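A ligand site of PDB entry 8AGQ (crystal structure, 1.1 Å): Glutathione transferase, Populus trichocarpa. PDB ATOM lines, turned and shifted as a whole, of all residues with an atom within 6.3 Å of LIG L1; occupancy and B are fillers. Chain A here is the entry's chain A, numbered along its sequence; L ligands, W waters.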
ATOM      1  N   PRO A   8     -14.747   7.025  12.407  1.00  0.00           N
ATOM      2  CA  PRO A   8     -15.909   7.693  12.969  1.00  0.00           C
ATOM      3  C   PRO A   8     -16.130   7.331  14.420  1.00  0.00           C
ATOM      4  O   PRO A   8     -15.993   6.157  14.794  1.00  0.00           O
ATOM      5  CB  PRO A   8     -17.099   7.132  12.155  1.00  0.00           C
ATOM      6  CG  PRO A   8     -16.508   6.441  11.006  1.00  0.00           C
ATOM      7  CD  PRO A   8     -15.107   6.048  11.375  1.00  0.00           C
ATOM      8  N   VAL A  10     -18.941   6.843  15.695  1.00  0.00           N
ATOM      9  CA  VAL A  10     -20.031   5.866  15.765  1.00  0.00           C
ATOM     10  C   VAL A  10     -19.593   4.445  15.414  1.00  0.00           C
ATOM     11  O   VAL A  10     -20.391   3.529  15.640  1.00  0.00           O
ATOM     12  CB  VAL A  10     -21.220   6.268  14.892  1.00  0.00           C
ATOM     13  CG1 VAL A  10     -21.878   7.561  15.375  1.00  0.00           C
ATOM     14  CG2 VAL A  10     -20.892   6.307  13.418  1.00  0.00           C
ATOM     15  N   ALA A  11     -18.413   4.255  14.828  1.00  0.00           N
ATOM     16  CA  ALA A  11     -18.093   2.927  14.313  1.00  0.00           C
ATOM     17  C   ALA A  11     -17.549   2.011  15.403  1.00  0.00           C
ATOM     18  O   ALA A  11     -16.839   2.414  16.326  1.00  0.00           O
ATOM     19  CB  ALA A  11     -17.103   3.084  13.160  1.00  0.00           C
ATOM     20  N   VAL A  12     -17.847   0.708  15.255  1.00  0.00           N
ATOM     21  CA  VAL A  12     -17.505  -0.274  16.259  1.00  0.00           C
ATOM     22  C   VAL A  12     -16.019  -0.349  16.578  1.00  0.00           C
ATOM     23  O   VAL A  12     -15.638  -0.386  17.747  1.00  0.00           O
ATOM     24  CB  VAL A  12     -18.070  -1.649  15.822  1.00  0.00           C
ATOM     25  CG1 VAL A  12     -17.403  -2.840  16.521  1.00  0.00           C
ATOM     26  CG2 VAL A  12     -19.582  -1.679  16.020  1.00  0.00           C
ATOM     27  N   CYS A  13     -15.146  -0.498  15.573  1.00  0.00           N
ATOM     28  CA  CYS A  13     -13.747  -0.797  15.905  1.00  0.00           C
ATOM     29  C   CYS A  13     -13.040   0.448  16.435  1.00  0.00           C
ATOM     30  O   CYS A  13     -12.257   0.365  17.381  1.00  0.00           O
ATOM     31  CB  CYS A  13     -12.967  -1.434  14.757  1.00  0.00           C
ATOM     32  SG  CYS A  13     -13.581  -3.060  14.261  1.00  0.00           S
ATOM     33  N   PRO A  14     -13.295   1.667  15.910  1.00  0.00           N
ATOM     34  CA  PRO A  14     -12.767   2.845  16.602  1.00  0.00           C
ATOM     35  C   PRO A  14     -13.260   2.929  18.049  1.00  0.00           C
ATOM     36  O   PRO A  14     -12.506   3.282  18.928  1.00  0.00           O
ATOM     37  CB  PRO A  14     -13.238   4.003  15.749  1.00  0.00           C
ATOM     38  CG  PRO A  14     -13.336   3.420  14.364  1.00  0.00           C
ATOM     39  CD  PRO A  14     -13.927   2.041  14.617  1.00  0.00           C
ATOM     40  N   ARG A  16     -13.979   0.480  20.053  1.00  0.00           N
ATOM     41  CA  ARG A  16     -13.270  -0.491  20.855  1.00  0.00           C
ATOM     42  C   ARG A  16     -11.968   0.126  21.377  1.00  0.00           C
ATOM     43  O   ARG A  16     -11.614  -0.013  22.554  1.00  0.00           O
ATOM     44  CB  ARG A  16     -13.007  -1.746  20.038  1.00  0.00           C
ATOM     45  CG  ARG A  16     -12.322  -2.870  20.759  1.00  0.00           C
ATOM     46  CD  ARG A  16     -12.213  -4.155  19.916  1.00  0.00           C
ATOM     47  NE  ARG A  16     -13.483  -4.721  19.477  1.00  0.00           N
ATOM     48  CZ  ARG A  16     -13.938  -4.758  18.258  1.00  0.00           C
ATOM     49  NH1 ARG A  16     -13.220  -4.369  17.238  1.00  0.00           N
ATOM     50  NH2 ARG A  16     -15.168  -5.179  18.041  1.00  0.00           N
ATOM     51  N   LEU A  35     -16.429   6.806   6.382  1.00  0.00           N
ATOM     52  CA  LEU A  35     -16.731   5.519   5.823  1.00  0.00           C
ATOM     53  C   LEU A  35     -17.925   5.596   4.881  1.00  0.00           C
ATOM     54  O   LEU A  35     -17.954   4.912   3.892  1.00  0.00           O
ATOM     55  CB  LEU A  35     -17.020   4.502   6.938  1.00  0.00           C
ATOM     56  CG  LEU A  35     -15.918   4.320   7.968  1.00  0.00           C
ATOM     57  CD1 LEU A  35     -16.294   3.225   8.932  1.00  0.00           C
ATOM     58  CD2 LEU A  35     -14.572   4.048   7.326  1.00  0.00           C
ATOM     59  N   ASP A  36     -18.873   6.490   5.164  1.00  0.00           N
ATOM     60  CA  ASP A  36     -20.056   6.612   4.328  1.00  0.00           C
ATOM     61  C   ASP A  36     -19.671   6.928   2.886  1.00  0.00           C
ATOM     62  O   ASP A  36     -20.315   6.450   1.945  1.00  0.00           O
ATOM     63  CB  ASP A  36     -21.000   7.726   4.807  1.00  0.00           C
ATOM     64  CG  ASP A  36     -21.783   7.394   6.073  1.00  0.00           C
ATOM     65  OD1 ASP A  36     -21.809   6.215   6.479  1.00  0.00           O
ATOM     66  OD2 ASP A  36     -22.441   8.284   6.629  1.00  0.00           O
ATOM     67  N   GLN A  40     -11.911   5.737   3.434  1.00  0.00           N
ATOM     68  CA  GLN A  40     -10.952   4.740   3.887  1.00  0.00           C
ATOM     69  C   GLN A  40     -10.345   3.949   2.747  1.00  0.00           C
ATOM     70  O   GLN A  40      -9.358   3.241   2.988  1.00  0.00           O
ATOM     71  CB  GLN A  40     -11.615   3.794   4.893  1.00  0.00           C
ATOM     72  CG  GLN A  40     -12.609   2.736   4.354  1.00  0.00           C
ATOM     73  CD  GLN A  40     -13.983   3.199   3.969  1.00  0.00           C
ATOM     74  OE1 GLN A  40     -14.254   4.392   3.819  1.00  0.00           O
ATOM     75  NE2 GLN A  40     -14.919   2.259   3.796  1.00  0.00           N
ATOM     76  N   ARG A  68      -7.808  -4.943  18.039  1.00  0.00           N
ATOM     77  CA  ARG A  68      -7.480  -5.774  19.203  1.00  0.00           C
ATOM     78  C   ARG A  68      -5.996  -5.752  19.500  1.00  0.00           C
ATOM     79  O   ARG A  68      -5.611  -5.971  20.639  1.00  0.00           O
ATOM     80  CB  ARG A  68      -8.075  -7.162  19.066  1.00  0.00           C
ATOM     81  CG  ARG A  68      -9.579  -7.098  18.923  1.00  0.00           C
ATOM     82  CD  ARG A  68     -10.219  -8.430  18.589  1.00  0.00           C
ATOM     83  NE  ARG A  68     -11.620  -8.310  18.234  1.00  0.00           N
ATOM     84  CZ  ARG A  68     -12.078  -7.940  17.042  1.00  0.00           C
ATOM     85  NH1 ARG A  68     -11.247  -7.581  16.062  1.00  0.00           N
ATOM     86  NH2 ARG A  68     -13.389  -7.954  16.858  1.00  0.00           N
ATOM     87  N   ASN A 108     -18.235 -11.922  17.059  1.00  0.00           N
ATOM     88  CA  ASN A 108     -18.273 -10.778  16.158  1.00  0.00           C
ATOM     89  C   ASN A 108     -18.572 -11.175  14.708  1.00  0.00           C
ATOM     90  O   ASN A 108     -19.159 -10.365  13.999  1.00  0.00           O
ATOM     91  CB  ASN A 108     -16.983  -9.968  16.191  1.00  0.00           C
ATOM     92  CG  ASN A 108     -17.210  -8.600  15.558  1.00  0.00           C
ATOM     93  OD1 ASN A 108     -18.020  -7.798  16.057  1.00  0.00           O
ATOM     94  ND2 ASN A 108     -16.493  -8.362  14.465  1.00  0.00           N
ATOM     95  N   VAL A 111     -22.327 -11.086  14.829  1.00  0.00           N
ATOM     96  CA  VAL A 111     -22.923  -9.781  15.093  1.00  0.00           C
ATOM     97  C   VAL A 111     -22.666  -8.828  13.926  1.00  0.00           C
ATOM     98  O   VAL A 111     -23.564  -8.089  13.507  1.00  0.00           O
ATOM     99  CB  VAL A 111     -22.405  -9.228  16.404  1.00  0.00           C
ATOM    100  CG1 VAL A 111     -22.895  -7.812  16.609  1.00  0.00           C
ATOM    101  CG2 VAL A 111     -22.804 -10.106  17.549  1.00  0.00           C
ATOM    102  N   PHE A 112     -21.436  -8.780  13.388  1.00  0.00           N
ATOM    103  CA  PHE A 112     -21.178  -7.917  12.228  1.00  0.00           C
ATOM    104  C   PHE A 112     -22.116  -8.282  11.091  1.00  0.00           C
ATOM    105  O   PHE A 112     -22.693  -7.352  10.456  1.00  0.00           O
ATOM    106  CB  PHE A 112     -19.732  -8.062  11.726  1.00  0.00           C
ATOM    107  CG  PHE A 112     -19.535  -7.390  10.376  1.00  0.00           C
ATOM    108  CD1 PHE A 112     -19.661  -6.010  10.224  1.00  0.00           C
ATOM    109  CD2 PHE A 112     -19.395  -8.150   9.229  1.00  0.00           C
ATOM    110  CE1 PHE A 112     -19.593  -5.415   8.989  1.00  0.00           C
ATOM    111  CE2 PHE A 112     -19.319  -7.566   7.990  1.00  0.00           C
ATOM    112  CZ  PHE A 112     -19.390  -6.204   7.887  1.00  0.00           C
ATOM    113  N   ASN A 113     -22.168  -9.544  10.709  1.00  0.00           N
ATOM    114  CA  ASN A 113     -23.021  -9.968   9.619  1.00  0.00           C
ATOM    115  C   ASN A 113     -24.442  -9.400   9.862  1.00  0.00           C
ATOM    116  O   ASN A 113     -24.978  -8.742   8.986  1.00  0.00           O
ATOM    117  CB  ASN A 113     -22.945 -11.483   9.373  1.00  0.00           C
ATOM    118  CG  ASN A 113     -21.630 -11.945   8.753  1.00  0.00           C
ATOM    119  OD1 ASN A 113     -20.825 -11.101   8.356  1.00  0.00           O
ATOM    120  ND2 ASN A 113     -21.345 -13.240   8.731  1.00  0.00           N
ATOM    121  N   VAL A 115     -25.599  -6.904  11.871  1.00  0.00           N
ATOM    122  CA  VAL A 115     -25.682  -5.444  11.839  1.00  0.00           C
ATOM    123  C   VAL A 115     -25.486  -4.922  10.415  1.00  0.00           C
ATOM    124  O   VAL A 115     -26.113  -3.938  10.012  1.00  0.00           O
ATOM    125  CB  VAL A 115     -24.733  -4.806  12.868  1.00  0.00           C
ATOM    126  CG1 VAL A 115     -24.702  -3.285  12.782  1.00  0.00           C
ATOM    127  CG2 VAL A 115     -25.071  -5.263  14.272  1.00  0.00           C
ATOM    128  N   PHE A 116     -24.595  -5.522   9.632  1.00  0.00           N
ATOM    129  CA  PHE A 116     -24.392  -5.093   8.252  1.00  0.00           C
ATOM    130  C   PHE A 116     -25.698  -5.216   7.469  1.00  0.00           C
ATOM    131  O   PHE A 116     -26.090  -4.278   6.765  1.00  0.00           O
ATOM    132  CB  PHE A 116     -23.267  -5.936   7.643  1.00  0.00           C
ATOM    133  CG  PHE A 116     -22.853  -5.434   6.296  1.00  0.00           C
ATOM    134  CD1 PHE A 116     -22.106  -4.250   6.166  1.00  0.00           C
ATOM    135  CD2 PHE A 116     -23.275  -6.046   5.118  1.00  0.00           C
ATOM    136  CE1 PHE A 116     -21.680  -3.783   4.930  1.00  0.00           C
ATOM    137  CE2 PHE A 116     -22.885  -5.552   3.867  1.00  0.00           C
ATOM    138  CZ  PHE A 116     -22.117  -4.418   3.786  1.00  0.00           C
ATOM    139  N   ILE A 120     -26.544  -1.394   8.320  1.00  0.00           N
ATOM    140  CA  ILE A 120     -25.672  -0.708   7.374  1.00  0.00           C
ATOM    141  C   ILE A 120     -26.294  -0.635   5.978  1.00  0.00           C
ATOM    142  O   ILE A 120     -26.296   0.442   5.355  1.00  0.00           O
ATOM    143  CB  ILE A 120     -24.263  -1.329   7.339  1.00  0.00           C
ATOM    144  CG1 ILE A 120     -23.605  -1.364   8.719  1.00  0.00           C
ATOM    145  CG2 ILE A 120     -23.354  -0.605   6.334  1.00  0.00           C
ATOM    146  CD1 ILE A 120     -23.420  -0.064   9.431  1.00  0.00           C
ATOM    147  N   ALA A 172     -20.099  -3.561  19.554  1.00  0.00           N
ATOM    148  CA  ALA A 172     -20.971  -4.344  18.685  1.00  0.00           C
ATOM    149  C   ALA A 172     -22.219  -4.764  19.434  1.00  0.00           C
ATOM    150  O   ALA A 172     -23.298  -4.849  18.845  1.00  0.00           O
ATOM    151  CB  ALA A 172     -20.277  -5.531  18.084  1.00  0.00           C
ATOM    152  N   TYR A 175     -24.903  -2.082  19.323  1.00  0.00           N
ATOM    153  CA  TYR A 175     -25.626  -2.096  18.047  1.00  0.00           C
ATOM    154  C   TYR A 175     -26.609  -3.269  17.978  1.00  0.00           C
ATOM    155  O   TYR A 175     -27.724  -3.136  17.482  1.00  0.00           O
ATOM    156  CB  TYR A 175     -24.687  -2.167  16.844  1.00  0.00           C
ATOM    157  CG  TYR A 175     -24.189  -0.820  16.377  1.00  0.00           C
ATOM    158  CD1 TYR A 175     -24.973   0.018  15.625  1.00  0.00           C
ATOM    159  CD2 TYR A 175     -22.928  -0.358  16.723  1.00  0.00           C
ATOM    160  CE1 TYR A 175     -24.544   1.247  15.184  1.00  0.00           C
ATOM    161  CE2 TYR A 175     -22.492   0.895  16.298  1.00  0.00           C
ATOM    162  CZ  TYR A 175     -23.283   1.709  15.530  1.00  0.00           C
ATOM    163  OH  TYR A 175     -22.903   2.954  15.077  1.00  0.00           O
HETATM  164  O1  LIG L   1     -18.926  -1.130   5.486  1.00  0.00           O
HETATM  165  C1  LIG L   1     -19.083  -0.697   6.775  1.00  0.00           C
HETATM  166  C2  LIG L   1     -19.290   0.658   7.003  1.00  0.00           C
HETATM  167  C3  LIG L   1     -19.426   1.090   8.285  1.00  0.00           C
HETATM  168  O2  LIG L   1     -19.697   2.393   8.560  1.00  0.00           O
HETATM  169  C4  LIG L   1     -19.399   0.205   9.373  1.00  0.00           C
HETATM  170  C5  LIG L   1     -19.491   0.711  10.792  1.00  0.00           C
HETATM  171  C6  LIG L   1     -19.027  -1.601   7.824  1.00  0.00           C
HETATM  172  C7  LIG L   1     -19.177  -1.136   9.112  1.00  0.00           C
HETATM  173  O3  LIG L   1     -19.210  -2.095  10.106  1.00  0.00           O
HETATM  174  C8  LIG L   1     -19.868  -1.688  11.363  1.00  0.00           C
HETATM  175  C9  LIG L   1     -19.189  -0.368  11.817  1.00  0.00           C
HETATM  176  O4  LIG L   1     -19.656   0.006  13.095  1.00  0.00           O
HETATM  177  C10 LIG L   1     -19.859  -2.865  12.300  1.00  0.00           C
HETATM  178  C11 LIG L   1     -18.679  -3.491  12.615  1.00  0.00           C
HETATM  179  C12 LIG L   1     -18.681  -4.616  13.423  1.00  0.00           C
HETATM  180  O5  LIG L   1     -17.548  -5.335  13.737  1.00  0.00           O
HETATM  181  C13 LIG L   1     -19.868  -5.045  14.002  1.00  0.00           C
HETATM  182  O6  LIG L   1     -19.915  -6.145  14.832  1.00  0.00           O
HETATM  183  C14 LIG L   1     -21.043  -4.395  13.703  1.00  0.00           C
HETATM  184  C15 LIG L   1     -21.031  -3.300  12.851  1.00  0.00           C
HETATM  185  N1  LG2 L   2      -9.911  -6.484  11.975  1.00  0.00           N
HETATM  186  C1  LG2 L   2     -10.086  -4.998  11.927  1.00  0.00           C
HETATM  187  C2  LG2 L   2      -9.854  -4.381  13.316  1.00  0.00           C
HETATM  188  O1  LG2 L   2      -9.337  -3.225  13.388  1.00  0.00           O
HETATM  189  O2  LG2 L   2     -10.239  -5.070  14.300  1.00  0.00           O
HETATM  190  C3  LG2 L   2     -11.495  -4.696  11.433  1.00  0.00           C
HETATM  191  C4  LG2 L   2     -11.619  -3.225  11.100  1.00  0.00           C
HETATM  192  C5  LG2 L   2     -12.960  -2.935  10.459  1.00  0.00           C
HETATM  193  O3  LG2 L   2     -13.692  -3.828  10.034  1.00  0.00           O
HETATM  194  N2  LG2 L   2     -13.327  -1.675  10.428  1.00  0.00           N
HETATM  195  C6  LG2 L   2     -14.577  -1.218   9.925  1.00  0.00           C
HETATM  196  C7  LG2 L   2     -14.366  -0.535   8.573  1.00  0.00           C
HETATM  197  O4  LG2 L   2     -13.372   0.163   8.369  1.00  0.00           O
HETATM  198  C8  LG2 L   2     -15.227  -0.252  10.935  1.00  0.00           C
HETATM  199  S1  LG2 L   2     -15.807  -1.080  12.440  1.00  0.00           S
HETATM  200  N3  LG2 L   2     -15.351  -0.682   7.711  1.00  0.00           N
HETATM  201  C9  LG2 L   2     -15.322  -0.120   6.382  1.00  0.00           C
HETATM  202  C10 LG2 L   2     -14.728  -1.029   5.313  1.00  0.00           C
HETATM  203  O5  LG2 L   2     -14.596  -0.522   4.181  1.00  0.00           O
HETATM  204  O6  LG2 L   2     -14.406  -2.189   5.646  1.00  0.00           O
HETATM  205  O   HOH W   1     -19.690   0.584   3.477  1.00  0.00           O
HETATM  206  O   HOH W   2     -15.746  -5.087  11.731  1.00  0.00           O
HETATM  207  O   HOH W   3     -20.451   3.789   6.465  1.00  0.00           O
HETATM  208  O   HOH W   4     -16.867  -3.527   9.441  1.00  0.00           O
HETATM  209  O   HOH W   5     -22.289   0.449  12.762  1.00  0.00           O
HETATM  210  O   HOH W   6     -18.191  -3.761   5.123  1.00  0.00           O
HETATM  211  O   HOH W   7     -19.747   4.092  10.857  1.00  0.00           O
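The side-chain amide oxygen (OD1) of Asn 108 is in hydrogen-bond range of an oxygen (O6) of LIG L1 (2.8 Å). The backbone NH (N) of Val 12 is in hydrogen-bond range of an oxygen (O4) of LIG L1, at 2.9 Å. N of Phe 112 lies within hydrogen-bond range of O6 of LIG L1. N of Cys 13 sits close to S1 of LG2 L2, 3.3 Å away. SG of Cys 13 sits close to S1 of LG2 L2 (3.5 Å). An oxygen (O5) of LG2 L2 sits at hydrogen-bond distance from the side-chain amide nitrogen (NE2) of Gln 40, 2.8 Å away. The guanidinium group of Arg 68 lies within salt-bridge range of an oxygen (O2) of LG2 L2 (3.2 Å).
The backbone carbonyl oxygen of Val 115 lies within hydrogen-bond range of the backbone NH of Ile 120, 3.1 Å away.
Ala 11 touches LIG L1. Leu 35 touches LIG L1 (CD1 to O2, 3.5 Å). Val 111 touches LIG L1. Val 115 touches LIG L1 (CG1 to C15, 3.7 Å). CE1 of Phe 116 touches O1 of LIG L1, 3.9 Å away. Ala 172 touches LIG L1. Hydrophobic or aromatic side chains that line LIG L1: Ala 11, Val 12, Leu 35, Val 111, Phe 112, Val 115, Phe 116 and Ala 172. Within 4 Å of LIG L1: Ala 11, Val 12, Leu 35, Asn 108, Val 111, Phe 112, Val 115, Phe 116 and Ala 172.
Water W3 bridges an oxygen (O2) of LIG L1 and the side-chain carboxylate (OD1) of Asp 36. Water W5 bridges an oxygen (O4) of LIG L1 (2.7 Å) and the side-chain hydroxyl of Tyr 175 (3.5 Å). Water W2 bridges an oxygen (O5) of LIG L1 (2.7 Å) and an oxygen (O3) of LG2 L2 (2.9 Å). Water W4 lies within hydrogen-bond range of an oxygen (O3) of LIG L1 (2.8 Å) and an oxygen (O3) of LG2 L2 (3.2 Å).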
